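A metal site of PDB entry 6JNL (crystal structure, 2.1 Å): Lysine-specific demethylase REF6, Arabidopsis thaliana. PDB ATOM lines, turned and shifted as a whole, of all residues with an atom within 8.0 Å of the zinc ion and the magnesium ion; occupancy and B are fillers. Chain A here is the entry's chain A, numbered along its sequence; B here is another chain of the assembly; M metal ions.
Gly 43 touches the magnesium ion (N to MG, 3.9 Å). Four residues have an atom within 4 Å of the magnesium ion: Cys 39, Trp 41, Gly 43 and Cys 44. The nearest printed residue that does not touch the magnesium ion is Pro 40 (4.01 Å).
Of the 18 residues printed, 4 come within 4 Å of the zinc ion. Along chain A the residues within 4 Å of the zinc ion span positions 39 to 61.
ND1 of His 57 is in hydrogen-bond range of OP1 of DT 4 of chain B (2.7 Å). The backbone NH of Trp 41 sits close to the side-chain sulfur of Cys 39 (3.3 Å). O of Met 46 is in hydrogen-bond range of N of Cys 39 (3.2 Å). The backbone NH (N) of Met 46 lies close to the side-chain sulfur (SG) of Cys 44 (3.6 Å).
The zinc ion is bound by a ring nitrogen (NE2) of His 57, a ring nitrogen (NE2) of His 61, the side-chain sulfur (SG) of Cys 39 and the side-chain sulfur (SG) of Cys 44.
The magnesium ion is bound by O of Trp 41 (2.4 Å) and O of Cys 39 (2.6 Å). Slightly farther from the magnesium ion lies the backbone carbonyl oxygen (O) of Cys 44 (2.8 Å).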
ATOM      1  N   LYS A  38      12.479 -23.893 -30.211  1.00  0.00           N
ATOM      2  CA  LYS A  38      12.214 -25.026 -31.097  1.00  0.00           C
ATOM      3  C   LYS A  38      11.778 -26.265 -30.276  1.00  0.00           C
ATOM      4  O   LYS A  38      12.112 -26.377 -29.102  1.00  0.00           O
ATOM      5  CB  LYS A  38      13.463 -25.375 -31.918  1.00  0.00           C
ATOM      6  CG  LYS A  38      14.099 -24.210 -32.674  1.00  0.00           C
ATOM      7  CD  LYS A  38      13.151 -23.617 -33.724  1.00  0.00           C
ATOM      8  CE  LYS A  38      13.196 -22.077 -33.889  1.00  0.00           C
ATOM      9  NZ  LYS A  38      13.992 -21.598 -35.043  1.00  0.00           N
ATOM     10  N   CYS A  39      11.006 -27.147 -30.888  1.00  0.00           N
ATOM     11  CA  CYS A  39      10.581 -28.369 -30.258  1.00  0.00           C
ATOM     12  C   CYS A  39      11.728 -29.342 -30.326  1.00  0.00           C
ATOM     13  O   CYS A  39      12.206 -29.614 -31.399  1.00  0.00           O
ATOM     14  CB  CYS A  39       9.358 -29.020 -30.928  1.00  0.00           C
ATOM     15  SG  CYS A  39       8.802 -30.505 -30.015  1.00  0.00           S
ATOM     16  N   PRO A  40      12.100 -29.950 -29.188  1.00  0.00           N
ATOM     17  CA  PRO A  40      13.178 -30.914 -29.230  1.00  0.00           C
ATOM     18  C   PRO A  40      12.745 -32.266 -29.732  1.00  0.00           C
ATOM     19  O   PRO A  40      13.552 -33.102 -29.862  1.00  0.00           O
ATOM     20  CB  PRO A  40      13.601 -31.019 -27.753  1.00  0.00           C
ATOM     21  CG  PRO A  40      12.324 -30.812 -27.026  1.00  0.00           C
ATOM     22  CD  PRO A  40      11.618 -29.757 -27.809  1.00  0.00           C
ATOM     23  N   TRP A  41      11.488 -32.500 -30.014  1.00  0.00           N
ATOM     24  CA  TRP A  41      11.138 -33.814 -30.538  1.00  0.00           C
ATOM     25  C   TRP A  41      11.580 -33.991 -31.973  1.00  0.00           C
ATOM     26  O   TRP A  41      11.542 -33.067 -32.809  1.00  0.00           O
ATOM     27  CB  TRP A  41       9.646 -34.015 -30.485  1.00  0.00           C
ATOM     28  CG  TRP A  41       9.188 -35.393 -30.462  1.00  0.00           C
ATOM     29  CD1 TRP A  41       8.776 -36.160 -31.533  1.00  0.00           C
ATOM     30  CD2 TRP A  41       9.035 -36.202 -29.311  1.00  0.00           C
ATOM     31  NE1 TRP A  41       8.346 -37.391 -31.090  1.00  0.00           N
ATOM     32  CE2 TRP A  41       8.505 -37.453 -29.729  1.00  0.00           C
ATOM     33  CE3 TRP A  41       9.289 -35.997 -27.957  1.00  0.00           C
ATOM     34  CZ2 TRP A  41       8.221 -38.469 -28.842  1.00  0.00           C
ATOM     35  CZ3 TRP A  41       9.002 -37.006 -27.065  1.00  0.00           C
ATOM     36  CH2 TRP A  41       8.469 -38.238 -27.514  1.00  0.00           C
ATOM     37  N   LYS A  42      11.965 -35.225 -32.228  1.00  0.00           N
ATOM     38  CA  LYS A  42      12.623 -35.625 -33.449  1.00  0.00           C
ATOM     39  C   LYS A  42      11.716 -35.340 -34.588  1.00  0.00           C
ATOM     40  O   LYS A  42      10.702 -35.992 -34.704  1.00  0.00           O
ATOM     41  CB  LYS A  42      12.851 -37.107 -33.386  1.00  0.00           C
ATOM     42  CG  LYS A  42      13.137 -37.827 -34.683  1.00  0.00           C
ATOM     43  CD  LYS A  42      14.552 -37.657 -35.130  1.00  0.00           C
ATOM     44  CE  LYS A  42      14.817 -38.807 -36.079  1.00  0.00           C
ATOM     45  NZ  LYS A  42      15.898 -38.372 -36.982  1.00  0.00           N
ATOM     46  N   GLY A  43      12.093 -34.364 -35.413  1.00  0.00           N
ATOM     47  CA  GLY A  43      11.357 -34.009 -36.603  1.00  0.00           C
ATOM     48  C   GLY A  43       9.981 -33.477 -36.293  1.00  0.00           C
ATOM     49  O   GLY A  43       9.052 -33.839 -36.928  1.00  0.00           O
ATOM     50  N   CYS A  44       9.870 -32.672 -35.258  1.00  0.00           N
ATOM     51  CA  CYS A  44       8.710 -31.844 -35.070  1.00  0.00           C
ATOM     52  C   CYS A  44       9.214 -30.447 -35.395  1.00  0.00           C
ATOM     53  O   CYS A  44      10.323 -30.074 -34.971  1.00  0.00           O
ATOM     54  CB  CYS A  44       8.194 -31.943 -33.634  1.00  0.00           C
ATOM     55  SG  CYS A  44       6.961 -30.701 -33.244  1.00  0.00           S
ATOM     56  N   LYS A  45       8.417 -29.699 -36.147  1.00  0.00           N
ATOM     57  CA  LYS A  45       8.843 -28.410 -36.734  1.00  0.00           C
ATOM     58  C   LYS A  45       8.253 -27.249 -36.004  1.00  0.00           C
ATOM     59  O   LYS A  45       8.580 -26.078 -36.292  1.00  0.00           O
ATOM     60  CB  LYS A  45       8.516 -28.391 -38.239  1.00  0.00           C
ATOM     61  CG  LYS A  45       9.616 -28.968 -39.155  1.00  0.00           C
ATOM     62  CD  LYS A  45      10.555 -29.986 -38.477  1.00  0.00           C
ATOM     63  CE  LYS A  45      11.819 -30.256 -39.262  1.00  0.00           C
ATOM     64  NZ  LYS A  45      11.477 -30.649 -40.655  1.00  0.00           N
ATOM     65  N   MET A  46       7.445 -27.553 -34.994  1.00  0.00           N
ATOM     66  CA  MET A  46       6.906 -26.507 -34.132  1.00  0.00           C
ATOM     67  C   MET A  46       7.974 -25.608 -33.523  1.00  0.00           C
ATOM     68  O   MET A  46       9.040 -26.074 -33.121  1.00  0.00           O
ATOM     69  CB  MET A  46       6.086 -27.116 -33.008  1.00  0.00           C
ATOM     70  CG  MET A  46       4.970 -26.239 -32.499  1.00  0.00           C
ATOM     71  SD  MET A  46       3.683 -26.160 -33.728  1.00  0.00           S
ATOM     72  CE  MET A  46       3.829 -27.600 -34.834  1.00  0.00           C
ATOM     73  N   THR A  47       7.643 -24.320 -33.417  1.00  0.00           N
ATOM     74  CA  THR A  47       8.513 -23.304 -32.913  1.00  0.00           C
ATOM     75  C   THR A  47       7.711 -22.388 -32.013  1.00  0.00           C
ATOM     76  O   THR A  47       6.522 -22.392 -32.119  1.00  0.00           O
ATOM     77  CB  THR A  47       9.101 -22.462 -34.048  1.00  0.00           C
ATOM     78  OG1 THR A  47       8.045 -21.762 -34.681  1.00  0.00           O
ATOM     79  CG2 THR A  47       9.798 -23.338 -35.038  1.00  0.00           C
ATOM     80  N   PHE A  48       8.352 -21.595 -31.171  1.00  0.00           N
ATOM     81  CA  PHE A  48       7.617 -20.864 -30.181  1.00  0.00           C
ATOM     82  C   PHE A  48       8.288 -19.573 -29.876  1.00  0.00           C
ATOM     83  O   PHE A  48       9.468 -19.413 -30.198  1.00  0.00           O
ATOM     84  CB  PHE A  48       7.586 -21.636 -28.842  1.00  0.00           C
ATOM     85  CG  PHE A  48       7.110 -23.030 -28.987  1.00  0.00           C
ATOM     86  CD1 PHE A  48       7.995 -24.032 -29.280  1.00  0.00           C
ATOM     87  CD2 PHE A  48       5.751 -23.309 -28.922  1.00  0.00           C
ATOM     88  CE1 PHE A  48       7.543 -25.292 -29.480  1.00  0.00           C
ATOM     89  CE2 PHE A  48       5.280 -24.574 -29.111  1.00  0.00           C
ATOM     90  CZ  PHE A  48       6.186 -25.557 -29.413  1.00  0.00           C
ATOM     91  N   ARG A  54       6.412 -23.962 -25.059  1.00  0.00           N
ATOM     92  CA  ARG A  54       7.228 -25.078 -25.484  1.00  0.00           C
ATOM     93  C   ARG A  54       7.173 -26.238 -24.446  1.00  0.00           C
ATOM     94  O   ARG A  54       7.091 -27.420 -24.810  1.00  0.00           O
ATOM     95  CB  ARG A  54       8.647 -24.616 -25.741  1.00  0.00           C
ATOM     96  CG  ARG A  54       9.695 -25.691 -26.042  1.00  0.00           C
ATOM     97  CD  ARG A  54      11.055 -25.049 -26.160  1.00  0.00           C
ATOM     98  NE  ARG A  54      12.081 -26.065 -26.330  1.00  0.00           N
ATOM     99  CZ  ARG A  54      12.661 -26.770 -25.339  1.00  0.00           C
ATOM    100  NH1 ARG A  54      12.345 -26.596 -24.043  1.00  0.00           N
ATOM    101  NH2 ARG A  54      13.593 -27.680 -25.627  1.00  0.00           N
ATOM    102  N   HIS A  57       3.903 -28.012 -24.647  1.00  0.00           N
ATOM    103  CA  HIS A  57       3.816 -28.687 -25.921  1.00  0.00           C
ATOM    104  C   HIS A  57       4.498 -30.049 -25.969  1.00  0.00           C
ATOM    105  O   HIS A  57       4.052 -30.945 -26.650  1.00  0.00           O
ATOM    106  CB  HIS A  57       4.345 -27.777 -27.047  1.00  0.00           C
ATOM    107  CG  HIS A  57       4.685 -28.526 -28.315  1.00  0.00           C
ATOM    108  ND1 HIS A  57       3.744 -28.862 -29.273  1.00  0.00           N
ATOM    109  CD2 HIS A  57       5.856 -29.047 -28.740  1.00  0.00           C
ATOM    110  CE1 HIS A  57       4.340 -29.487 -30.262  1.00  0.00           C
ATOM    111  NE2 HIS A  57       5.615 -29.607 -29.962  1.00  0.00           N
ATOM    112  N   ILE A  58       5.582 -30.222 -25.250  1.00  0.00           N
ATOM    113  CA  ILE A  58       6.344 -31.496 -25.355  1.00  0.00           C
ATOM    114  C   ILE A  58       5.456 -32.641 -24.867  1.00  0.00           C
ATOM    115  O   ILE A  58       5.627 -33.741 -25.324  1.00  0.00           O
ATOM    116  CB  ILE A  58       7.686 -31.425 -24.588  1.00  0.00           C
ATOM    117  CG1 ILE A  58       8.694 -30.474 -25.300  1.00  0.00           C
ATOM    118  CG2 ILE A  58       8.333 -32.806 -24.404  1.00  0.00           C
ATOM    119  CD1 ILE A  58       9.708 -29.805 -24.328  1.00  0.00           C
ATOM    120  N   ARG A  59       4.505 -32.338 -23.955  1.00  0.00           N
ATOM    121  CA  ARG A  59       3.556 -33.304 -23.426  1.00  0.00           C
ATOM    122  C   ARG A  59       2.605 -33.818 -24.450  1.00  0.00           C
ATOM    123  O   ARG A  59       2.103 -34.961 -24.333  1.00  0.00           O
ATOM    124  CB  ARG A  59       2.769 -32.778 -22.205  1.00  0.00           C
ATOM    125  CG  ARG A  59       3.681 -32.264 -21.079  1.00  0.00           C
ATOM    126  CD  ARG A  59       2.892 -31.712 -19.937  1.00  0.00           C
ATOM    127  NE  ARG A  59       3.560 -30.671 -19.135  1.00  0.00           N
ATOM    128  CZ  ARG A  59       3.041 -29.510 -18.755  1.00  0.00           C
ATOM    129  NH1 ARG A  59       1.793 -29.143 -19.094  1.00  0.00           N
ATOM    130  NH2 ARG A  59       3.757 -28.690 -17.946  1.00  0.00           N
ATOM    131  N   VAL A  60       2.398 -33.056 -25.512  1.00  0.00           N
ATOM    132  CA  VAL A  60       1.615 -33.670 -26.557  1.00  0.00           C
ATOM    133  C   VAL A  60       2.425 -34.837 -27.129  1.00  0.00           C
ATOM    134  O   VAL A  60       1.844 -35.820 -27.526  1.00  0.00           O
ATOM    135  CB  VAL A  60       0.976 -32.739 -27.632  1.00  0.00           C
ATOM    136  CG1 VAL A  60       0.690 -31.337 -27.101  1.00  0.00           C
ATOM    137  CG2 VAL A  60       1.730 -32.669 -28.918  1.00  0.00           C
ATOM    138  N   HIS A  61       3.748 -34.761 -27.148  1.00  0.00           N
ATOM    139  CA  HIS A  61       4.551 -35.867 -27.674  1.00  0.00           C
ATOM    140  C   HIS A  61       4.612 -36.970 -26.678  1.00  0.00           C
ATOM    141  O   HIS A  61       4.420 -38.076 -27.031  1.00  0.00           O
ATOM    142  CB  HIS A  61       5.926 -35.407 -28.064  1.00  0.00           C
ATOM    143  CG  HIS A  61       5.934 -34.461 -29.227  1.00  0.00           C
ATOM    144  ND1 HIS A  61       5.504 -34.829 -30.477  1.00  0.00           N
ATOM    145  CD2 HIS A  61       6.390 -33.178 -29.349  1.00  0.00           C
ATOM    146  CE1 HIS A  61       5.674 -33.826 -31.325  1.00  0.00           C
ATOM    147  NE2 HIS A  61       6.222 -32.822 -30.673  1.00  0.00           N
ATOM    148  P    DT B   4       0.450 -27.249 -28.075  1.00  0.00           P
ATOM    149  OP1  DT B   4       1.360 -27.634 -29.118  1.00  0.00           O
ATOM    150  OP2  DT B   4       0.855 -27.414 -26.664  1.00  0.00           O
ATOM    151  O5'  DT B   4       0.051 -25.734 -28.197  1.00  0.00           O
ATOM    152  C5'  DT B   4      -0.334 -25.219 -29.489  1.00  0.00           C
ATOM    153  C4'  DT B   4      -0.527 -23.724 -29.385  1.00  0.00           C
ATOM    154  O4'  DT B   4      -1.577 -23.520 -28.417  1.00  0.00           O
ATOM    155  C3'  DT B   4       0.684 -22.933 -28.868  1.00  0.00           C
ATOM    156  O3'  DT B   4       0.805 -21.719 -29.650  1.00  0.00           O
ATOM    157  C2'  DT B   4       0.337 -22.651 -27.422  1.00  0.00           C
ATOM    158  C1'  DT B   4      -1.179 -22.523 -27.512  1.00  0.00           C
ATOM    159  N1   DT B   4      -1.879 -22.774 -26.251  1.00  0.00           N
ATOM    160  C2   DT B   4      -2.795 -21.860 -25.760  1.00  0.00           C
ATOM    161  O2   DT B   4      -3.058 -20.812 -26.305  1.00  0.00           O
ATOM    162  N3   DT B   4      -3.356 -22.215 -24.561  1.00  0.00           N
ATOM    163  C4   DT B   4      -3.102 -23.361 -23.824  1.00  0.00           C
ATOM    164  O4   DT B   4      -3.674 -23.535 -22.757  1.00  0.00           O
ATOM    165  C5   DT B   4      -2.160 -24.279 -24.423  1.00  0.00           C
ATOM    166  C7   DT B   4      -1.848 -25.558 -23.699  1.00  0.00           C
ATOM    167  C6   DT B   4      -1.602 -23.950 -25.588  1.00  0.00           C
HETATM  168 ZN    ZN M   1       6.843 -30.884 -30.971  1.00  0.00          ZN
HETATM  169 MG    MG M   2      12.591 -30.997 -33.534  1.00  0.00          MG
